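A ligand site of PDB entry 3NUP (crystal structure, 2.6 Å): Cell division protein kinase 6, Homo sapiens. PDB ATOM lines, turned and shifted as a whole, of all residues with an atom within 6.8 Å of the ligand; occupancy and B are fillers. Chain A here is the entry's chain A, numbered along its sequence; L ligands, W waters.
Residues that only touch the ligand: Glu 99, Ile 19, Val 27, Gln 149, Leu 152, Ala 41, Asp 163, His 100 and Gln 103.
Hydrophobic or aromatic side chains within 4 Å of the ligand: Ile 19, Val 27, Ala 41 and Leu 152.
12 residues have an atom within 4 Å of the ligand: Ile 19, Val 27, Ala 41, Lys 43, Glu 99, His 100, Val 101, Gln 103, Asp 104, Gln 149, Leu 152 and Asp 163.
Water W1 lies within hydrogen-bond range of the backbone carbonyl oxygen (O) of Gln 149 and the side-chain carboxylate (OD2) of Asp 104.
The side-chain carboxylate of Asp 104 is in hydrogen-bond range of the backbone NH of Thr 107 (2.9 Å).
N of Gly 20 lies within hydrogen-bond range of O of Val 27, at 3.0 Å.
The side-chain amino group of Lys 43 lies within salt-bridge range of the side-chain carboxylate of Asp 163, 3.3 Å away.
N of Ala 41 lies within hydrogen-bond range of O of Phe 98, at 2.9 Å.
The side-chain carboxylate (OE1) of Glu 99 is in hydrogen-bond range of the backbone NH (N) of Arg 78, 2.9 Å away.
The backbone carbonyl oxygen (O) of Val 27 sits at hydrogen-bond distance from the backbone NH (N) of Ile 19.
The backbone NH (N) of Val 153 is in hydrogen-bond range of the backbone carbonyl oxygen (O) of Gln 103 (2.9 Å).
A nitrogen (N1) of the ligand sits close to the side-chain amino group (NZ) of Lys 43, at 3.2 Å.
N of Val 101 lies within hydrogen-bond range of N3 of the ligand, at 3.3 Å.
The backbone carbonyl oxygen (O) of Val 101 lies within hydrogen-bond range of a nitrogen (N5) of the ligand (2.8 Å).
The side-chain carboxylate (OD2) of Asp 104 is in salt-bridge range of a nitrogen (N6) of the ligand.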
ATOM      1  N   ILE A  19      18.662 -11.255  -0.831  1.00  0.00           N
ATOM      2  CA  ILE A  19      17.937 -10.714  -1.973  1.00  0.00           C
ATOM      3  C   ILE A  19      18.085  -9.199  -2.048  1.00  0.00           C
ATOM      4  O   ILE A  19      18.652  -8.662  -3.008  1.00  0.00           O
ATOM      5  CB  ILE A  19      16.449 -10.974  -1.885  1.00  0.00           C
ATOM      6  CG1 ILE A  19      16.159 -12.455  -1.663  1.00  0.00           C
ATOM      7  CG2 ILE A  19      15.823 -10.465  -3.161  1.00  0.00           C
ATOM      8  CD1 ILE A  19      14.858 -12.702  -0.875  1.00  0.00           C
ATOM      9  N   GLY A  20      17.555  -8.511  -1.045  1.00  0.00           N
ATOM     10  CA  GLY A  20      17.660  -7.066  -1.007  1.00  0.00           C
ATOM     11  C   GLY A  20      18.542  -6.629   0.146  1.00  0.00           C
ATOM     12  O   GLY A  20      19.286  -5.645   0.047  1.00  0.00           O
ATOM     13  N   GLY A  25      15.800  -1.854   4.650  1.00  0.00           N
ATOM     14  CA  GLY A  25      16.849  -2.764   5.054  1.00  0.00           C
ATOM     15  C   GLY A  25      17.192  -3.796   3.998  1.00  0.00           C
ATOM     16  O   GLY A  25      16.804  -3.656   2.838  1.00  0.00           O
ATOM     17  N   VAL A  27      16.844  -7.642   2.622  1.00  0.00           N
ATOM     18  CA  VAL A  27      15.974  -8.823   2.638  1.00  0.00           C
ATOM     19  C   VAL A  27      16.642 -10.153   2.328  1.00  0.00           C
ATOM     20  O   VAL A  27      17.319 -10.310   1.311  1.00  0.00           O
ATOM     21  CB  VAL A  27      14.841  -8.685   1.642  1.00  0.00           C
ATOM     22  CG1 VAL A  27      13.887  -9.876   1.790  1.00  0.00           C
ATOM     23  CG2 VAL A  27      14.137  -7.361   1.843  1.00  0.00           C
ATOM     24  N   VAL A  40      10.597 -18.079   3.787  1.00  0.00           N
ATOM     25  CA  VAL A  40      10.132 -16.799   4.310  1.00  0.00           C
ATOM     26  C   VAL A  40      11.121 -15.728   3.859  1.00  0.00           C
ATOM     27  O   VAL A  40      12.186 -16.049   3.318  1.00  0.00           O
ATOM     28  CB  VAL A  40      10.038 -16.809   5.856  1.00  0.00           C
ATOM     29  CG1 VAL A  40       8.852 -17.636   6.299  1.00  0.00           C
ATOM     30  CG2 VAL A  40      11.313 -17.341   6.458  1.00  0.00           C
ATOM     31  N   ALA A  41      10.770 -14.464   4.067  1.00  0.00           N
ATOM     32  CA  ALA A  41      11.645 -13.354   3.711  1.00  0.00           C
ATOM     33  C   ALA A  41      11.928 -12.572   4.976  1.00  0.00           C
ATOM     34  O   ALA A  41      11.046 -11.930   5.524  1.00  0.00           O
ATOM     35  CB  ALA A  41      10.961 -12.468   2.683  1.00  0.00           C
ATOM     36  N   LYS A  43      13.614  -9.535   6.863  1.00  0.00           N
ATOM     37  CA  LYS A  43      14.164  -8.214   6.643  1.00  0.00           C
ATOM     38  C   LYS A  43      14.776  -7.769   7.960  1.00  0.00           C
ATOM     39  O   LYS A  43      14.101  -7.764   8.989  1.00  0.00           O
ATOM     40  CB  LYS A  43      13.065  -7.229   6.210  1.00  0.00           C
ATOM     41  CG  LYS A  43      13.594  -5.826   5.945  1.00  0.00           C
ATOM     42  CD  LYS A  43      12.479  -4.871   5.593  1.00  0.00           C
ATOM     43  CE  LYS A  43      11.819  -5.239   4.282  1.00  0.00           C
ATOM     44  NZ  LYS A  43      10.725  -4.285   3.924  1.00  0.00           N
ATOM     45  N   VAL A  77       1.504  -8.650   1.469  1.00  0.00           N
ATOM     46  CA  VAL A  77       2.295  -9.773   1.965  1.00  0.00           C
ATOM     47  C   VAL A  77       2.043 -10.035   3.441  1.00  0.00           C
ATOM     48  O   VAL A  77       1.959  -9.112   4.236  1.00  0.00           O
ATOM     49  CB  VAL A  77       3.821  -9.603   1.785  1.00  0.00           C
ATOM     50  CG1 VAL A  77       4.186  -9.707   0.331  1.00  0.00           C
ATOM     51  CG2 VAL A  77       4.289  -8.298   2.387  1.00  0.00           C
ATOM     52  N   ARG A  78       1.911 -11.314   3.775  1.00  0.00           N
ATOM     53  CA  ARG A  78       1.687 -11.730   5.141  1.00  0.00           C
ATOM     54  C   ARG A  78       2.926 -11.423   5.962  1.00  0.00           C
ATOM     55  O   ARG A  78       4.039 -11.602   5.495  1.00  0.00           O
ATOM     56  CB  ARG A  78       1.433 -13.246   5.219  1.00  0.00           C
ATOM     57  CG  ARG A  78       0.091 -13.721   4.660  1.00  0.00           C
ATOM     58  CD  ARG A  78      -1.088 -13.347   5.570  1.00  0.00           C
ATOM     59  NE  ARG A  78      -1.454 -11.941   5.498  1.00  0.00           N
ATOM     60  CZ  ARG A  78      -2.008 -11.361   4.425  1.00  0.00           C
ATOM     61  NH1 ARG A  78      -2.258 -12.061   3.323  1.00  0.00           N
ATOM     62  NH2 ARG A  78      -2.326 -10.073   4.453  1.00  0.00           N
ATOM     63  N   PHE A  98       8.314 -12.222   6.696  1.00  0.00           N
ATOM     64  CA  PHE A  98       7.171 -12.222   5.780  1.00  0.00           C
ATOM     65  C   PHE A  98       7.064 -13.525   5.008  1.00  0.00           C
ATOM     66  O   PHE A  98       8.031 -14.265   4.908  1.00  0.00           O
ATOM     67  CB  PHE A  98       7.326 -11.095   4.748  1.00  0.00           C
ATOM     68  CG  PHE A  98       7.350  -9.714   5.327  1.00  0.00           C
ATOM     69  CD1 PHE A  98       6.172  -9.081   5.691  1.00  0.00           C
ATOM     70  CD2 PHE A  98       8.546  -9.025   5.457  1.00  0.00           C
ATOM     71  CE1 PHE A  98       6.186  -7.782   6.160  1.00  0.00           C
ATOM     72  CE2 PHE A  98       8.567  -7.715   5.931  1.00  0.00           C
ATOM     73  CZ  PHE A  98       7.385  -7.101   6.285  1.00  0.00           C
ATOM     74  N   GLU A  99       5.894 -13.800   4.452  1.00  0.00           N
ATOM     75  CA  GLU A  99       5.782 -15.003   3.652  1.00  0.00           C
ATOM     76  C   GLU A  99       6.721 -14.701   2.499  1.00  0.00           C
ATOM     77  O   GLU A  99       6.995 -13.537   2.230  1.00  0.00           O
ATOM     78  CB  GLU A  99       4.362 -15.204   3.118  1.00  0.00           C
ATOM     79  CG  GLU A  99       3.752 -13.979   2.514  1.00  0.00           C
ATOM     80  CD  GLU A  99       2.448 -14.290   1.824  1.00  0.00           C
ATOM     81  OE1 GLU A  99       1.559 -13.407   1.771  1.00  0.00           O
ATOM     82  OE2 GLU A  99       2.320 -15.428   1.328  1.00  0.00           O
ATOM     83  N   HIS A 100       7.198 -15.718   1.810  1.00  0.00           N
ATOM     84  CA  HIS A 100       8.095 -15.499   0.692  1.00  0.00           C
ATOM     85  C   HIS A 100       7.374 -15.788  -0.620  1.00  0.00           C
ATOM     86  O   HIS A 100       6.718 -16.820  -0.754  1.00  0.00           O
ATOM     87  CB  HIS A 100       9.344 -16.384   0.861  1.00  0.00           C
ATOM     88  CG  HIS A 100      10.257 -16.369  -0.333  1.00  0.00           C
ATOM     89  ND1 HIS A 100       9.949 -17.013  -1.519  1.00  0.00           N
ATOM     90  CD2 HIS A 100      11.430 -15.733  -0.549  1.00  0.00           C
ATOM     91  CE1 HIS A 100      10.886 -16.776  -2.405  1.00  0.00           C
ATOM     92  NE2 HIS A 100      11.798 -15.997  -1.856  1.00  0.00           N
ATOM     93  N   VAL A 101       7.470 -14.864  -1.571  1.00  0.00           N
ATOM     94  CA  VAL A 101       6.852 -15.026  -2.877  1.00  0.00           C
ATOM     95  C   VAL A 101       8.025 -15.164  -3.859  1.00  0.00           C
ATOM     96  O   VAL A 101       8.977 -14.401  -3.803  1.00  0.00           O
ATOM     97  CB  VAL A 101       5.946 -13.821  -3.209  1.00  0.00           C
ATOM     98  CG1 VAL A 101       5.235 -14.049  -4.515  1.00  0.00           C
ATOM     99  CG2 VAL A 101       4.943 -13.602  -2.089  1.00  0.00           C
ATOM    100  N   ASP A 102       7.958 -16.151  -4.730  1.00  0.00           N
ATOM    101  CA  ASP A 102       9.039 -16.435  -5.661  1.00  0.00           C
ATOM    102  C   ASP A 102       9.364 -15.355  -6.645  1.00  0.00           C
ATOM    103  O   ASP A 102      10.515 -15.251  -7.077  1.00  0.00           O
ATOM    104  CB  ASP A 102       8.770 -17.733  -6.448  1.00  0.00           C
ATOM    105  CG  ASP A 102       8.654 -18.962  -5.548  1.00  0.00           C
ATOM    106  OD1 ASP A 102       9.577 -19.225  -4.738  1.00  0.00           O
ATOM    107  OD2 ASP A 102       7.635 -19.693  -5.652  1.00  0.00           O
ATOM    108  N   GLN A 103       8.385 -14.544  -7.026  1.00  0.00           N
ATOM    109  CA  GLN A 103       8.662 -13.513  -8.036  1.00  0.00           C
ATOM    110  C   GLN A 103       7.899 -12.186  -7.911  1.00  0.00           C
ATOM    111  O   GLN A 103       6.905 -12.089  -7.205  1.00  0.00           O
ATOM    112  CB  GLN A 103       8.427 -14.126  -9.433  1.00  0.00           C
ATOM    113  CG  GLN A 103       6.979 -14.396  -9.788  1.00  0.00           C
ATOM    114  CD  GLN A 103       6.848 -15.189 -11.073  1.00  0.00           C
ATOM    115  OE1 GLN A 103       7.577 -14.950 -12.034  1.00  0.00           O
ATOM    116  NE2 GLN A 103       5.887 -16.128 -11.104  1.00  0.00           N
ATOM    117  N   ASP A 104       8.414 -11.170  -8.607  1.00  0.00           N
ATOM    118  CA  ASP A 104       7.798  -9.858  -8.619  1.00  0.00           C
ATOM    119  C   ASP A 104       7.297  -9.506 -10.009  1.00  0.00           C
ATOM    120  O   ASP A 104       7.531 -10.250 -10.957  1.00  0.00           O
ATOM    121  CB  ASP A 104       8.753  -8.769  -8.138  1.00  0.00           C
ATOM    122  CG  ASP A 104      10.059  -8.736  -8.890  1.00  0.00           C
ATOM    123  OD1 ASP A 104      10.073  -9.009 -10.113  1.00  0.00           O
ATOM    124  OD2 ASP A 104      11.084  -8.428  -8.246  1.00  0.00           O
ATOM    125  N   THR A 107       9.952  -9.589 -12.944  1.00  0.00           N
ATOM    126  CA  THR A 107      10.259 -10.949 -13.399  1.00  0.00           C
ATOM    127  C   THR A 107       9.100 -11.505 -14.209  1.00  0.00           C
ATOM    128  O   THR A 107       9.288 -12.166 -15.239  1.00  0.00           O
ATOM    129  CB  THR A 107      10.497 -11.870 -12.195  1.00  0.00           C
ATOM    130  OG1 THR A 107      11.562 -11.353 -11.394  1.00  0.00           O
ATOM    131  CG2 THR A 107      10.856 -13.258 -12.656  1.00  0.00           C
ATOM    132  N   GLN A 149       9.223  -3.887  -8.703  1.00  0.00           N
ATOM    133  CA  GLN A 149      10.050  -4.727  -7.836  1.00  0.00           C
ATOM    134  C   GLN A 149       9.448  -5.069  -6.476  1.00  0.00           C
ATOM    135  O   GLN A 149       9.851  -6.041  -5.838  1.00  0.00           O
ATOM    136  CB  GLN A 149      11.436  -4.100  -7.602  1.00  0.00           C
ATOM    137  CG  GLN A 149      12.300  -3.961  -8.846  1.00  0.00           C
ATOM    138  CD  GLN A 149      11.890  -2.769  -9.690  1.00  0.00           C
ATOM    139  OE1 GLN A 149      11.615  -1.692  -9.172  1.00  0.00           O
ATOM    140  NE2 GLN A 149      11.839  -2.969 -11.009  1.00  0.00           N
ATOM    141  N   ASN A 150       8.489  -4.259  -6.005  1.00  0.00           N
ATOM    142  CA  ASN A 150       7.884  -4.575  -4.711  1.00  0.00           C
ATOM    143  C   ASN A 150       6.372  -4.853  -4.766  1.00  0.00           C
ATOM    144  O   ASN A 150       5.629  -4.640  -3.795  1.00  0.00           O
ATOM    145  CB  ASN A 150       8.229  -3.532  -3.661  1.00  0.00           C
ATOM    146  CG  ASN A 150       7.829  -2.146  -4.059  1.00  0.00           C
ATOM    147  OD1 ASN A 150       6.762  -1.946  -4.622  1.00  0.00           O
ATOM    148  ND2 ASN A 150       8.686  -1.171  -3.763  1.00  0.00           N
ATOM    149  N   ILE A 151       5.957  -5.313  -5.932  1.00  0.00           N
ATOM    150  CA  ILE A 151       4.604  -5.744  -6.211  1.00  0.00           C
ATOM    151  C   ILE A 151       4.877  -7.224  -6.547  1.00  0.00           C
ATOM    152  O   ILE A 151       5.287  -7.539  -7.649  1.00  0.00           O
ATOM    153  CB  ILE A 151       4.042  -5.048  -7.439  1.00  0.00           C
ATOM    154  CG1 ILE A 151       3.692  -3.591  -7.107  1.00  0.00           C
ATOM    155  CG2 ILE A 151       2.824  -5.800  -7.956  1.00  0.00           C
ATOM    156  CD1 ILE A 151       3.066  -2.852  -8.240  1.00  0.00           C
ATOM    157  N   LEU A 152       4.700  -8.130  -5.590  1.00  0.00           N
ATOM    158  CA  LEU A 152       4.977  -9.541  -5.798  1.00  0.00           C
ATOM    159  C   LEU A 152       3.818 -10.331  -6.441  1.00  0.00           C
ATOM    160  O   LEU A 152       2.647 -10.033  -6.221  1.00  0.00           O
ATOM    161  CB  LEU A 152       5.342 -10.176  -4.476  1.00  0.00           C
ATOM    162  CG  LEU A 152       6.189  -9.251  -3.602  1.00  0.00           C
ATOM    163  CD1 LEU A 152       6.331  -9.818  -2.212  1.00  0.00           C
ATOM    164  CD2 LEU A 152       7.540  -9.061  -4.248  1.00  0.00           C
ATOM    165  N   VAL A 153       4.160 -11.321  -7.267  1.00  0.00           N
ATOM    166  CA  VAL A 153       3.165 -12.155  -7.929  1.00  0.00           C
ATOM    167  C   VAL A 153       3.269 -13.581  -7.384  1.00  0.00           C
ATOM    168  O   VAL A 153       4.316 -14.228  -7.536  1.00  0.00           O
ATOM    169  CB  VAL A 153       3.386 -12.168  -9.449  1.00  0.00           C
ATOM    170  CG1 VAL A 153       2.270 -12.961 -10.104  1.00  0.00           C
ATOM    171  CG2 VAL A 153       3.447 -10.758  -9.997  1.00  0.00           C
ATOM    172  N   ALA A 162       4.394  -5.211  -1.238  1.00  0.00           N
ATOM    173  CA  ALA A 162       5.436  -5.444  -0.234  1.00  0.00           C
ATOM    174  C   ALA A 162       6.266  -4.178  -0.033  1.00  0.00           C
ATOM    175  O   ALA A 162       6.039  -3.161  -0.669  1.00  0.00           O
ATOM    176  CB  ALA A 162       6.328  -6.598  -0.695  1.00  0.00           C
ATOM    177  N   ASP A 163       7.214  -4.254   0.903  1.00  0.00           N
ATOM    178  CA  ASP A 163       8.139  -3.151   1.144  1.00  0.00           C
ATOM    179  C   ASP A 163       7.535  -1.764   1.435  1.00  0.00           C
ATOM    180  O   ASP A 163       8.001  -0.765   0.881  1.00  0.00           O
ATOM    181  CB  ASP A 163       9.065  -3.030  -0.078  1.00  0.00           C
ATOM    182  CG  ASP A 163      10.444  -2.517   0.260  1.00  0.00           C
ATOM    183  OD1 ASP A 163      11.315  -2.541  -0.632  1.00  0.00           O
ATOM    184  OD2 ASP A 163      10.646  -2.086   1.419  1.00  0.00           O
ATOM    185  N   PHE A 164       6.527  -1.716   2.315  1.00  0.00           N
ATOM    186  CA  PHE A 164       5.859  -0.462   2.690  1.00  0.00           C
ATOM    187  C   PHE A 164       5.750  -0.376   4.210  1.00  0.00           C
ATOM    188  O   PHE A 164       5.911  -1.377   4.905  1.00  0.00           O
ATOM    189  CB  PHE A 164       4.438  -0.406   2.094  1.00  0.00           C
ATOM    190  CG  PHE A 164       3.556  -1.539   2.544  1.00  0.00           C
ATOM    191  CD1 PHE A 164       2.897  -1.484   3.780  1.00  0.00           C
ATOM    192  CD2 PHE A 164       3.416  -2.691   1.766  1.00  0.00           C
ATOM    193  CE1 PHE A 164       2.136  -2.539   4.228  1.00  0.00           C
ATOM    194  CE2 PHE A 164       2.659  -3.759   2.217  1.00  0.00           C
ATOM    195  CZ  PHE A 164       2.015  -3.685   3.449  1.00  0.00           C
HETATM  196  C1  LIG L   1      10.154  -8.140   0.402  1.00  0.00           C
HETATM  197  N1  LIG L   1      10.569  -6.288   1.477  1.00  0.00           N
HETATM  198  C2  LIG L   1       9.896  -7.441   1.574  1.00  0.00           C
HETATM  199  N2  LIG L   1      11.259  -6.155   0.309  1.00  0.00           N
HETATM  200  C3  LIG L   1      11.009  -7.275  -0.343  1.00  0.00           C
HETATM  201  N3  LIG L   1       8.606 -11.958  -0.564  1.00  0.00           N
HETATM  202  C4  LIG L   1       9.492 -11.357  -1.317  1.00  0.00           C
HETATM  203  N4  LIG L   1      10.035 -10.140  -1.069  1.00  0.00           N
HETATM  204  C5  LIG L   1       9.586  -9.504   0.083  1.00  0.00           C
HETATM  205  N5  LIG L   1       9.840 -12.089  -2.425  1.00  0.00           N
HETATM  206  C6  LIG L   1       8.644 -10.080   0.944  1.00  0.00           C
HETATM  207  N6  LIG L   1      12.299 -10.512  -5.480  1.00  0.00           N
HETATM  208  C7  LIG L   1       8.192 -11.336   0.550  1.00  0.00           C
HETATM  209  C8  LIG L   1      11.667  -7.440  -1.718  1.00  0.00           C
HETATM  210  C9  LIG L   1      11.225  -6.324  -2.652  1.00  0.00           C
HETATM  211  C10 LIG L   1      13.188  -7.445  -1.630  1.00  0.00           C
HETATM  212  C11 LIG L   1      10.830 -11.973  -3.504  1.00  0.00           C
HETATM  213  C12 LIG L   1      10.084 -11.419  -4.738  1.00  0.00           C
HETATM  214  C13 LIG L   1      11.106 -11.347  -5.907  1.00  0.00           C
HETATM  215  C14 LIG L   1      12.979 -11.010  -4.293  1.00  0.00           C
HETATM  216  C15 LIG L   1      12.023 -11.054  -3.114  1.00  0.00           C
HETATM  217  C16 LIG L   1      13.258 -10.466  -6.600  1.00  0.00           C
HETATM  218  O   HOH W   1      12.318  -6.986  -5.636  1.00  0.00           O
